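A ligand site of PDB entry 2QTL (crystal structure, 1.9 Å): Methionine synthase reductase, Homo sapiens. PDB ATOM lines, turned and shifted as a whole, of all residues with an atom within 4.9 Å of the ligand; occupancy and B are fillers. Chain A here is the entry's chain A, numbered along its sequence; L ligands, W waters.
Water W7 lies within hydrogen-bond range of O2 of the ligand (2.5 Å) and NH2 of Arg 292 (3.4 Å). Water W1 lies within hydrogen-bond range of an oxygen (O7) of the ligand and the backbone carbonyl oxygen (O) of Asn 312. Water W4 lies within hydrogen-bond range of O of Ser 295 (2.7 Å), O8 of the ligand (2.7 Å) and N of Val 310 (2.8 Å). Water W8 lies within hydrogen-bond range of O1 of the ligand (2.9 Å) and NH1 of Arg 218 (2.9 Å). Water W3 bridges O10 of the ligand (2.9 Å) and O of Trp 538 (3.4 Å).
The backbone NH of Val 314 sits at hydrogen-bond distance from the side-chain hydroxyl of Thr 331 (3.0 Å). OH of Tyr 294 lies within hydrogen-bond range of SG of Cys 330 (3.5 Å). The indole nitrogen (NE1) of Trp 538 lies close to the side-chain hydroxyl (OG) of Ser 295, 3.5 Å away. The side-chain hydroxyl of Ser 295 lies within hydrogen-bond range of the side-chain carboxylate of Asp 536. O of Val 314 sits at hydrogen-bond distance from N of Gly 328 (2.8 Å). The side-chain carboxylate (OD2) of Asp 536 is in hydrogen-bond range of the indole nitrogen (NE1) of Trp 538, at 3.1 Å.
Residues that only touch the ligand: CSO 262, Phe 311, Gly 328, Arg 366, Asn 312, Phe 316, Val 314 and Asp 536. Hydrophobic or aromatic side chains that line the ligand: Pro 293, Tyr 294, Phe 311, Val 314, Phe 316, Val 329 and Trp 538. Of the 23 residues printed, 17 come within 4 Å of the ligand. The nearest printed residue that does not touch the ligand is Ala 153 (4.1 Å).
O of Pro 293 is in hydrogen-bond range of O9 of the ligand (2.6 Å). N of Thr 331 lies within hydrogen-bond range of O14 of the ligand, at 2.9 Å. OG1 of Thr 331 lies within hydrogen-bond range of O14 of the ligand (2.6 Å). N of Cys 330 lies within hydrogen-bond range of O13 of the ligand (2.8 Å). The side-chain hydroxyl (OH) of Tyr 294 sits at hydrogen-bond distance from an oxygen (O11) of the ligand (2.8 Å). N of Ser 295 sits at hydrogen-bond distance from O8 of the ligand (2.8 Å). The side-chain hydroxyl (OG) of Ser 295 sits at hydrogen-bond distance from a nitrogen (N3) of the ligand, at 3.2 Å. O of Val 310 is in hydrogen-bond range of N2 of the ligand. An oxygen (O1) of the ligand is in hydrogen-bond range of the backbone NH (N) of Val 329 (2.9 Å). The guanidinium group (NE) of Arg 292 is in salt-bridge range of an oxygen (O13) of the ligand, 2.9 Å away. The indole nitrogen (NE1) of Trp 538 lies close to a nitrogen (N3) of the ligand, 3.5 Å away.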
ATOM      1  N   ALA A 153     -13.642  -8.575 -10.183  1.00  0.00           N
ATOM      2  CA  ALA A 153     -14.993  -8.212 -10.618  1.00  0.00           C
ATOM      3  C   ALA A 153     -15.531  -7.145  -9.640  1.00  0.00           C
ATOM      4  O   ALA A 153     -15.048  -7.015  -8.510  1.00  0.00           O
ATOM      5  CB  ALA A 153     -15.933  -9.442 -10.608  1.00  0.00           C
ATOM      6  N   ARG A 218     -38.643  -8.489 -13.470  1.00  0.00           N
ATOM      7  CA  ARG A 218     -38.437  -9.449 -14.554  1.00  0.00           C
ATOM      8  C   ARG A 218     -38.524 -10.941 -14.166  1.00  0.00           C
ATOM      9  O   ARG A 218     -38.546 -11.823 -15.044  1.00  0.00           O
ATOM     10  CB  ARG A 218     -37.067  -9.172 -15.208  1.00  0.00           C
ATOM     11  CG  ARG A 218     -37.045  -7.864 -16.027  1.00  0.00           C
ATOM     12  CD  ARG A 218     -37.634  -8.098 -17.408  1.00  0.00           C
ATOM     13  NE  ARG A 218     -37.395  -6.963 -18.307  1.00  0.00           N
ATOM     14  CZ  ARG A 218     -36.312  -6.799 -19.045  1.00  0.00           C
ATOM     15  NH1 ARG A 218     -35.343  -7.722 -19.065  1.00  0.00           N
ATOM     16  NH2 ARG A 218     -36.232  -5.746 -19.830  1.00  0.00           N
ATOM     17  N   CSO A 262     -39.605 -17.005 -20.847  1.00  0.00           N
ATOM     18  CA  CSO A 262     -39.172 -15.924 -19.973  1.00  0.00           C
ATOM     19  CB  CSO A 262     -38.016 -15.120 -20.552  1.00  0.00           C
ATOM     20  SG  CSO A 262     -36.660 -16.223 -20.859  1.00  0.00           S
ATOM     21  C   CSO A 262     -40.297 -14.973 -19.575  1.00  0.00           C
ATOM     22  O   CSO A 262     -40.097 -13.769 -19.551  1.00  0.00           O
ATOM     23  OD  CSO A 262     -35.900 -16.601 -19.303  1.00  0.00           O
ATOM     24  N   ARG A 292     -25.453  -6.517 -10.895  1.00  0.00           N
ATOM     25  CA  ARG A 292     -24.806  -7.388 -11.887  1.00  0.00           C
ATOM     26  C   ARG A 292     -23.281  -7.156 -11.813  1.00  0.00           C
ATOM     27  O   ARG A 292     -22.840  -6.029 -11.847  1.00  0.00           O
ATOM     28  CB  ARG A 292     -25.322  -7.124 -13.333  1.00  0.00           C
ATOM     29  CG  ARG A 292     -26.587  -7.951 -13.750  1.00  0.00           C
ATOM     30  CD  ARG A 292     -27.840  -7.565 -12.921  1.00  0.00           C
ATOM     31  NE  ARG A 292     -29.039  -8.034 -13.645  1.00  0.00           N
ATOM     32  CZ  ARG A 292     -30.247  -8.159 -13.122  1.00  0.00           C
ATOM     33  NH1 ARG A 292     -30.454  -7.856 -11.836  1.00  0.00           N
ATOM     34  NH2 ARG A 292     -31.242  -8.587 -13.898  1.00  0.00           N
ATOM     35  N   PRO A 293     -22.503  -8.237 -11.669  1.00  0.00           N
ATOM     36  CA  PRO A 293     -21.041  -8.143 -11.692  1.00  0.00           C
ATOM     37  C   PRO A 293     -20.476  -8.052 -13.091  1.00  0.00           C
ATOM     38  O   PRO A 293     -21.035  -8.664 -14.044  1.00  0.00           O
ATOM     39  CB  PRO A 293     -20.572  -9.451 -11.033  1.00  0.00           C
ATOM     40  CG  PRO A 293     -21.656 -10.460 -11.385  1.00  0.00           C
ATOM     41  CD  PRO A 293     -22.953  -9.608 -11.362  1.00  0.00           C
ATOM     42  N   TYR A 294     -19.426  -7.271 -13.209  1.00  0.00           N
ATOM     43  CA  TYR A 294     -18.614  -7.176 -14.430  1.00  0.00           C
ATOM     44  C   TYR A 294     -17.141  -7.372 -14.095  1.00  0.00           C
ATOM     45  O   TYR A 294     -16.699  -7.053 -12.969  1.00  0.00           O
ATOM     46  CB  TYR A 294     -18.873  -5.866 -15.213  1.00  0.00           C
ATOM     47  CG  TYR A 294     -20.316  -5.891 -15.683  1.00  0.00           C
ATOM     48  CD1 TYR A 294     -20.664  -6.547 -16.865  1.00  0.00           C
ATOM     49  CD2 TYR A 294     -21.328  -5.391 -14.869  1.00  0.00           C
ATOM     50  CE1 TYR A 294     -21.986  -6.645 -17.265  1.00  0.00           C
ATOM     51  CE2 TYR A 294     -22.668  -5.529 -15.222  1.00  0.00           C
ATOM     52  CZ  TYR A 294     -22.977  -6.149 -16.428  1.00  0.00           C
ATOM     53  OH  TYR A 294     -24.277  -6.285 -16.743  1.00  0.00           O
ATOM     54  N   SER A 295     -16.373  -7.857 -15.086  1.00  0.00           N
ATOM     55  CA  SER A 295     -14.925  -8.044 -14.883  1.00  0.00           C
ATOM     56  C   SER A 295     -14.102  -6.822 -15.226  1.00  0.00           C
ATOM     57  O   SER A 295     -14.429  -6.121 -16.190  1.00  0.00           O
ATOM     58  CB  SER A 295     -14.405  -9.267 -15.683  1.00  0.00           C
ATOM     59  OG  SER A 295     -15.249 -10.373 -15.373  1.00  0.00           O
ATOM     60  N   VAL A 310     -16.285  -4.574 -20.243  1.00  0.00           N
ATOM     61  CA  VAL A 310     -16.767  -4.927 -21.596  1.00  0.00           C
ATOM     62  C   VAL A 310     -17.968  -5.818 -21.434  1.00  0.00           C
ATOM     63  O   VAL A 310     -17.934  -6.779 -20.646  1.00  0.00           O
ATOM     64  CB  VAL A 310     -15.679  -5.756 -22.359  1.00  0.00           C
ATOM     65  CG1 VAL A 310     -16.193  -6.174 -23.738  1.00  0.00           C
ATOM     66  CG2 VAL A 310     -14.409  -4.947 -22.515  1.00  0.00           C
ATOM     67  N   PHE A 311     -19.032  -5.567 -22.204  1.00  0.00           N
ATOM     68  CA  PHE A 311     -20.225  -6.417 -22.086  1.00  0.00           C
ATOM     69  C   PHE A 311     -20.992  -6.494 -23.394  1.00  0.00           C
ATOM     70  O   PHE A 311     -20.975  -5.522 -24.171  1.00  0.00           O
ATOM     71  CB  PHE A 311     -21.163  -5.911 -20.963  1.00  0.00           C
ATOM     72  CG  PHE A 311     -21.638  -4.510 -21.149  1.00  0.00           C
ATOM     73  CD1 PHE A 311     -22.824  -4.242 -21.874  1.00  0.00           C
ATOM     74  CD2 PHE A 311     -20.892  -3.474 -20.647  1.00  0.00           C
ATOM     75  CE1 PHE A 311     -23.281  -2.917 -22.022  1.00  0.00           C
ATOM     76  CE2 PHE A 311     -21.301  -2.167 -20.806  1.00  0.00           C
ATOM     77  CZ  PHE A 311     -22.494  -1.869 -21.481  1.00  0.00           C
ATOM     78  N   ASN A 312     -21.584  -7.666 -23.660  1.00  0.00           N
ATOM     79  CA  ASN A 312     -22.535  -7.733 -24.766  1.00  0.00           C
ATOM     80  C   ASN A 312     -23.876  -7.270 -24.230  1.00  0.00           C
ATOM     81  O   ASN A 312     -24.220  -7.578 -23.083  1.00  0.00           O
ATOM     82  CB  ASN A 312     -22.745  -9.213 -25.168  1.00  0.00           C
ATOM     83  CG  ASN A 312     -21.632  -9.756 -26.064  1.00  0.00           C
ATOM     84  OD1 ASN A 312     -21.105  -9.044 -26.905  1.00  0.00           O
ATOM     85  ND2 ASN A 312     -21.292 -11.043 -25.894  1.00  0.00           N
ATOM     86  N   VAL A 314     -27.431  -7.905 -23.727  1.00  0.00           N
ATOM     87  CA  VAL A 314     -28.223  -9.134 -23.804  1.00  0.00           C
ATOM     88  C   VAL A 314     -29.580  -8.812 -24.437  1.00  0.00           C
ATOM     89  O   VAL A 314     -30.220  -7.792 -24.111  1.00  0.00           O
ATOM     90  CB  VAL A 314     -28.407  -9.792 -22.415  1.00  0.00           C
ATOM     91  CG1 VAL A 314     -29.495 -10.906 -22.426  1.00  0.00           C
ATOM     92  CG2 VAL A 314     -27.078 -10.268 -21.873  1.00  0.00           C
ATOM     93  N   PHE A 316     -33.139 -11.093 -25.739  1.00  0.00           N
ATOM     94  CA  PHE A 316     -33.736 -12.418 -25.724  1.00  0.00           C
ATOM     95  C   PHE A 316     -35.216 -12.318 -26.143  1.00  0.00           C
ATOM     96  O   PHE A 316     -35.799 -11.236 -26.076  1.00  0.00           O
ATOM     97  CB  PHE A 316     -33.599 -13.046 -24.318  1.00  0.00           C
ATOM     98  CG  PHE A 316     -34.304 -12.251 -23.210  1.00  0.00           C
ATOM     99  CD1 PHE A 316     -35.569 -12.638 -22.757  1.00  0.00           C
ATOM    100  CD2 PHE A 316     -33.699 -11.115 -22.635  1.00  0.00           C
ATOM    101  CE1 PHE A 316     -36.235 -11.906 -21.761  1.00  0.00           C
ATOM    102  CE2 PHE A 316     -34.355 -10.384 -21.644  1.00  0.00           C
ATOM    103  CZ  PHE A 316     -35.600 -10.784 -21.190  1.00  0.00           C
ATOM    104  N   GLY A 328     -31.539  -7.150 -21.668  1.00  0.00           N
ATOM    105  CA  GLY A 328     -31.214  -7.462 -20.287  1.00  0.00           C
ATOM    106  C   GLY A 328     -31.465  -6.221 -19.437  1.00  0.00           C
ATOM    107  O   GLY A 328     -31.422  -5.102 -19.957  1.00  0.00           O
ATOM    108  N   VAL A 329     -31.686  -6.393 -18.132  1.00  0.00           N
ATOM    109  CA  VAL A 329     -31.952  -5.243 -17.263  1.00  0.00           C
ATOM    110  C   VAL A 329     -30.712  -4.327 -17.198  1.00  0.00           C
ATOM    111  O   VAL A 329     -30.813  -3.108 -17.381  1.00  0.00           O
ATOM    112  CB  VAL A 329     -32.342  -5.707 -15.851  1.00  0.00           C
ATOM    113  CG1 VAL A 329     -32.492  -4.508 -14.886  1.00  0.00           C
ATOM    114  CG2 VAL A 329     -33.602  -6.548 -15.933  1.00  0.00           C
ATOM    115  N   CYS A 330     -29.538  -4.900 -16.896  1.00  0.00           N
ATOM    116  CA  CYS A 330     -28.394  -4.040 -16.586  1.00  0.00           C
ATOM    117  C   CYS A 330     -27.797  -3.582 -17.903  1.00  0.00           C
ATOM    118  O   CYS A 330     -27.501  -2.427 -18.068  1.00  0.00           O
ATOM    119  CB  CYS A 330     -27.338  -4.799 -15.749  1.00  0.00           C
ATOM    120  SG  CYS A 330     -26.063  -3.698 -15.152  1.00  0.00           S
ATOM    121  N   THR A 331     -27.617  -4.503 -18.862  1.00  0.00           N
ATOM    122  CA  THR A 331     -26.981  -4.104 -20.125  1.00  0.00           C
ATOM    123  C   THR A 331     -27.880  -3.187 -20.980  1.00  0.00           C
ATOM    124  O   THR A 331     -27.359  -2.328 -21.682  1.00  0.00           O
ATOM    125  CB  THR A 331     -26.436  -5.342 -20.938  1.00  0.00           C
ATOM    126  OG1 THR A 331     -27.505  -6.257 -21.188  1.00  0.00           O
ATOM    127  CG2 THR A 331     -25.380  -6.102 -20.079  1.00  0.00           C
ATOM    128  N   GLY A 332     -29.191  -3.407 -20.949  1.00  0.00           N
ATOM    129  CA  GLY A 332     -30.190  -2.452 -21.570  1.00  0.00           C
ATOM    130  C   GLY A 332     -30.064  -1.036 -21.018  1.00  0.00           C
ATOM    131  O   GLY A 332     -30.001  -0.052 -21.770  1.00  0.00           O
ATOM    132  N   ARG A 366     -16.077  -6.488  -5.119  1.00  0.00           N
ATOM    133  CA  ARG A 366     -16.271  -7.817  -4.601  1.00  0.00           C
ATOM    134  C   ARG A 366     -15.082  -8.034  -3.663  1.00  0.00           C
ATOM    135  O   ARG A 366     -13.934  -7.725  -4.008  1.00  0.00           O
ATOM    136  CB  ARG A 366     -16.292  -8.829  -5.757  1.00  0.00           C
ATOM    137  CG  ARG A 366     -16.383 -10.263  -5.295  1.00  0.00           C
ATOM    138  CD  ARG A 366     -16.629 -11.188  -6.463  1.00  0.00           C
ATOM    139  NE  ARG A 366     -15.414 -11.398  -7.235  1.00  0.00           N
ATOM    140  CZ  ARG A 366     -15.326 -12.209  -8.285  1.00  0.00           C
ATOM    141  NH1 ARG A 366     -16.383 -12.896  -8.701  1.00  0.00           N
ATOM    142  NH2 ARG A 366     -14.159 -12.338  -8.895  1.00  0.00           N
ATOM    143  N   THR A 388     -16.593 -12.011 -25.351  1.00  0.00           N
ATOM    144  CA  THR A 388     -16.324 -11.034 -24.297  1.00  0.00           C
ATOM    145  C   THR A 388     -15.511 -11.607 -23.125  1.00  0.00           C
ATOM    146  O   THR A 388     -15.007 -10.840 -22.294  1.00  0.00           O
ATOM    147  CB  THR A 388     -17.604 -10.388 -23.777  1.00  0.00           C
ATOM    148  OG1 THR A 388     -18.505 -11.416 -23.400  1.00  0.00           O
ATOM    149  CG2 THR A 388     -18.270  -9.578 -24.866  1.00  0.00           C
ATOM    150  N   ALA A 391     -12.181 -10.127 -21.911  1.00  0.00           N
ATOM    151  CA  ALA A 391     -12.141  -8.912 -21.070  1.00  0.00           C
ATOM    152  C   ALA A 391     -11.055  -8.877 -19.972  1.00  0.00           C
ATOM    153  O   ALA A 391     -10.232  -7.953 -19.976  1.00  0.00           O
ATOM    154  CB  ALA A 391     -13.519  -8.681 -20.445  1.00  0.00           C
ATOM    155  N   ASP A 536     -13.403 -18.100 -14.709  1.00  0.00           N
ATOM    156  CA  ASP A 536     -14.308 -16.996 -14.433  1.00  0.00           C
ATOM    157  C   ASP A 536     -15.432 -17.130 -15.461  1.00  0.00           C
ATOM    158  O   ASP A 536     -15.381 -16.596 -16.542  1.00  0.00           O
ATOM    159  CB  ASP A 536     -13.593 -15.666 -14.532  1.00  0.00           C
ATOM    160  CG  ASP A 536     -14.483 -14.467 -14.154  1.00  0.00           C
ATOM    161  OD1 ASP A 536     -15.442 -14.612 -13.368  1.00  0.00           O
ATOM    162  OD2 ASP A 536     -14.221 -13.354 -14.627  1.00  0.00           O
ATOM    163  N   ILE A 537     -16.447 -17.907 -15.094  1.00  0.00           N
ATOM    164  CA  ILE A 537     -17.547 -18.253 -15.980  1.00  0.00           C
ATOM    165  C   ILE A 537     -18.742 -17.380 -15.614  1.00  0.00           C
ATOM    166  O   ILE A 537     -19.023 -17.163 -14.415  1.00  0.00           O
ATOM    167  CB  ILE A 537     -17.894 -19.764 -15.842  1.00  0.00           C
ATOM    168  CG1 ILE A 537     -16.628 -20.613 -16.082  1.00  0.00           C
ATOM    169  CG2 ILE A 537     -19.030 -20.213 -16.801  1.00  0.00           C
ATOM    170  CD1 ILE A 537     -15.821 -20.239 -17.401  1.00  0.00           C
ATOM    171  N   TRP A 538     -19.447 -16.872 -16.621  1.00  0.00           N
ATOM    172  CA  TRP A 538     -20.352 -15.725 -16.407  1.00  0.00           C
ATOM    173  C   TRP A 538     -21.795 -16.083 -16.432  1.00  0.00           C
ATOM    174  O   TRP A 538     -22.635 -15.235 -16.104  1.00  0.00           O
ATOM    175  CB  TRP A 538     -20.085 -14.619 -17.431  1.00  0.00           C
ATOM    176  CG  TRP A 538     -18.742 -13.968 -17.253  1.00  0.00           C
ATOM    177  CD1 TRP A 538     -17.933 -14.090 -16.183  1.00  0.00           C
ATOM    178  CD2 TRP A 538     -18.063 -13.094 -18.176  1.00  0.00           C
ATOM    179  NE1 TRP A 538     -16.800 -13.340 -16.352  1.00  0.00           N
ATOM    180  CE2 TRP A 538     -16.847 -12.723 -17.579  1.00  0.00           C
ATOM    181  CE3 TRP A 538     -18.394 -12.554 -19.419  1.00  0.00           C
ATOM    182  CZ2 TRP A 538     -15.945 -11.837 -18.181  1.00  0.00           C
ATOM    183  CZ3 TRP A 538     -17.480 -11.710 -20.031  1.00  0.00           C
ATOM    184  CH2 TRP A 538     -16.279 -11.348 -19.417  1.00  0.00           C
HETATM  185  P1  LIG L   1     -30.564 -10.057 -17.383  1.00  0.00           P
HETATM  186  O1  LIG L   1     -31.755  -9.162 -17.334  1.00  0.00           O
HETATM  187  O2  LIG L   1     -30.154 -10.554 -16.026  1.00  0.00           O
HETATM  188  O3  LIG L   1     -30.870 -11.305 -18.363  1.00  0.00           O
HETATM  189  C1  LIG L   1     -32.000 -11.611 -19.133  1.00  0.00           C
HETATM  190  C2  LIG L   1     -32.172 -13.107 -18.807  1.00  0.00           C
HETATM  191  O4  LIG L   1     -33.474 -13.653 -19.024  1.00  0.00           O
HETATM  192  C3  LIG L   1     -31.187 -14.024 -19.502  1.00  0.00           C
HETATM  193  O5  LIG L   1     -29.882 -13.990 -18.949  1.00  0.00           O
HETATM  194  C4  LIG L   1     -31.860 -15.331 -19.146  1.00  0.00           C
HETATM  195  O6  LIG L   1     -31.695 -15.598 -17.767  1.00  0.00           O
HETATM  196  C5  LIG L   1     -33.330 -15.008 -19.390  1.00  0.00           C
HETATM  197  N1  LIG L   1     -20.976 -10.219 -18.485  1.00  0.00           N
HETATM  198  C6  LIG L   1     -20.344  -9.369 -19.379  1.00  0.00           C
HETATM  199  O7  LIG L   1     -20.910  -9.084 -20.427  1.00  0.00           O
HETATM  200  N2  LIG L   1     -19.093  -8.831 -19.053  1.00  0.00           N
HETATM  201  C7  LIG L   1     -18.448  -9.124 -17.875  1.00  0.00           C
HETATM  202  O8  LIG L   1     -17.330  -8.582 -17.622  1.00  0.00           O
HETATM  203  C8  LIG L   1     -19.066  -9.996 -16.990  1.00  0.00           C
HETATM  204  N3  LIG L   1     -18.432 -10.328 -15.801  1.00  0.00           N
HETATM  205  C9  LIG L   1     -19.059 -11.208 -14.935  1.00  0.00           C
HETATM  206  C10 LIG L   1     -18.429 -11.530 -13.732  1.00  0.00           C
HETATM  207  C11 LIG L   1     -19.035 -12.414 -12.842  1.00  0.00           C
HETATM  208  C12 LIG L   1     -18.274 -12.720 -11.574  1.00  0.00           C
HETATM  209  C13 LIG L   1     -20.288 -12.984 -13.138  1.00  0.00           C
HETATM  210  C14 LIG L   1     -20.985 -13.938 -12.184  1.00  0.00           C
HETATM  211  C15 LIG L   1     -20.952 -12.647 -14.324  1.00  0.00           C
HETATM  212  C16 LIG L   1     -20.347 -11.742 -15.222  1.00  0.00           C
HETATM  213  N4  LIG L   1     -20.984 -11.369 -16.406  1.00  0.00           N
HETATM  214  C17 LIG L   1     -20.341 -10.532 -17.273  1.00  0.00           C
HETATM  215  C18 LIG L   1     -22.527 -11.414 -16.528  1.00  0.00           C
HETATM  216  C19 LIG L   1     -23.238 -10.159 -15.991  1.00  0.00           C
HETATM  217  O9  LIG L   1     -23.122 -10.146 -14.560  1.00  0.00           O
HETATM  218  C20 LIG L   1     -24.725 -10.100 -16.389  1.00  0.00           C
HETATM  219  O10 LIG L   1     -25.317 -11.345 -16.116  1.00  0.00           O
HETATM  220  C21 LIG L   1     -24.894  -9.898 -17.905  1.00  0.00           C
HETATM  221  O11 LIG L   1     -24.394  -8.637 -18.213  1.00  0.00           O
HETATM  222  C22 LIG L   1     -26.384  -9.871 -18.250  1.00  0.00           C
HETATM  223  O12 LIG L   1     -27.113  -9.035 -17.303  1.00  0.00           O
HETATM  224  P2  LIG L   1     -28.421  -8.233 -17.730  1.00  0.00           P
HETATM  225  O13 LIG L   1     -29.031  -7.580 -16.515  1.00  0.00           O
HETATM  226  O14 LIG L   1     -28.279  -7.325 -18.897  1.00  0.00           O
HETATM  227  O15 LIG L   1     -29.388  -9.415 -18.284  1.00  0.00           O
HETATM  228  O   HOH W   1     -23.533  -9.129 -20.836  1.00  0.00           O
HETATM  229  O   HOH W   2     -24.249 -12.353 -13.020  1.00  0.00           O
HETATM  230  O   HOH W   3     -24.951 -13.598 -17.895  1.00  0.00           O
HETATM  231  O   HOH W   4     -15.534  -6.768 -18.588  1.00  0.00           O
HETATM  232  O   HOH W   5     -35.692 -12.286 -18.136  1.00  0.00           O
HETATM  233  O   HOH W   6     -27.757 -11.403 -14.961  1.00  0.00           O
HETATM  234  O   HOH W   7     -31.347 -11.949 -14.269  1.00  0.00           O
HETATM  235  O   HOH W   8     -34.510 -10.029 -17.437  1.00  0.00           O
HETATM  236  O   HOH W   9     -22.193 -12.375 -20.003  1.00  0.00           O
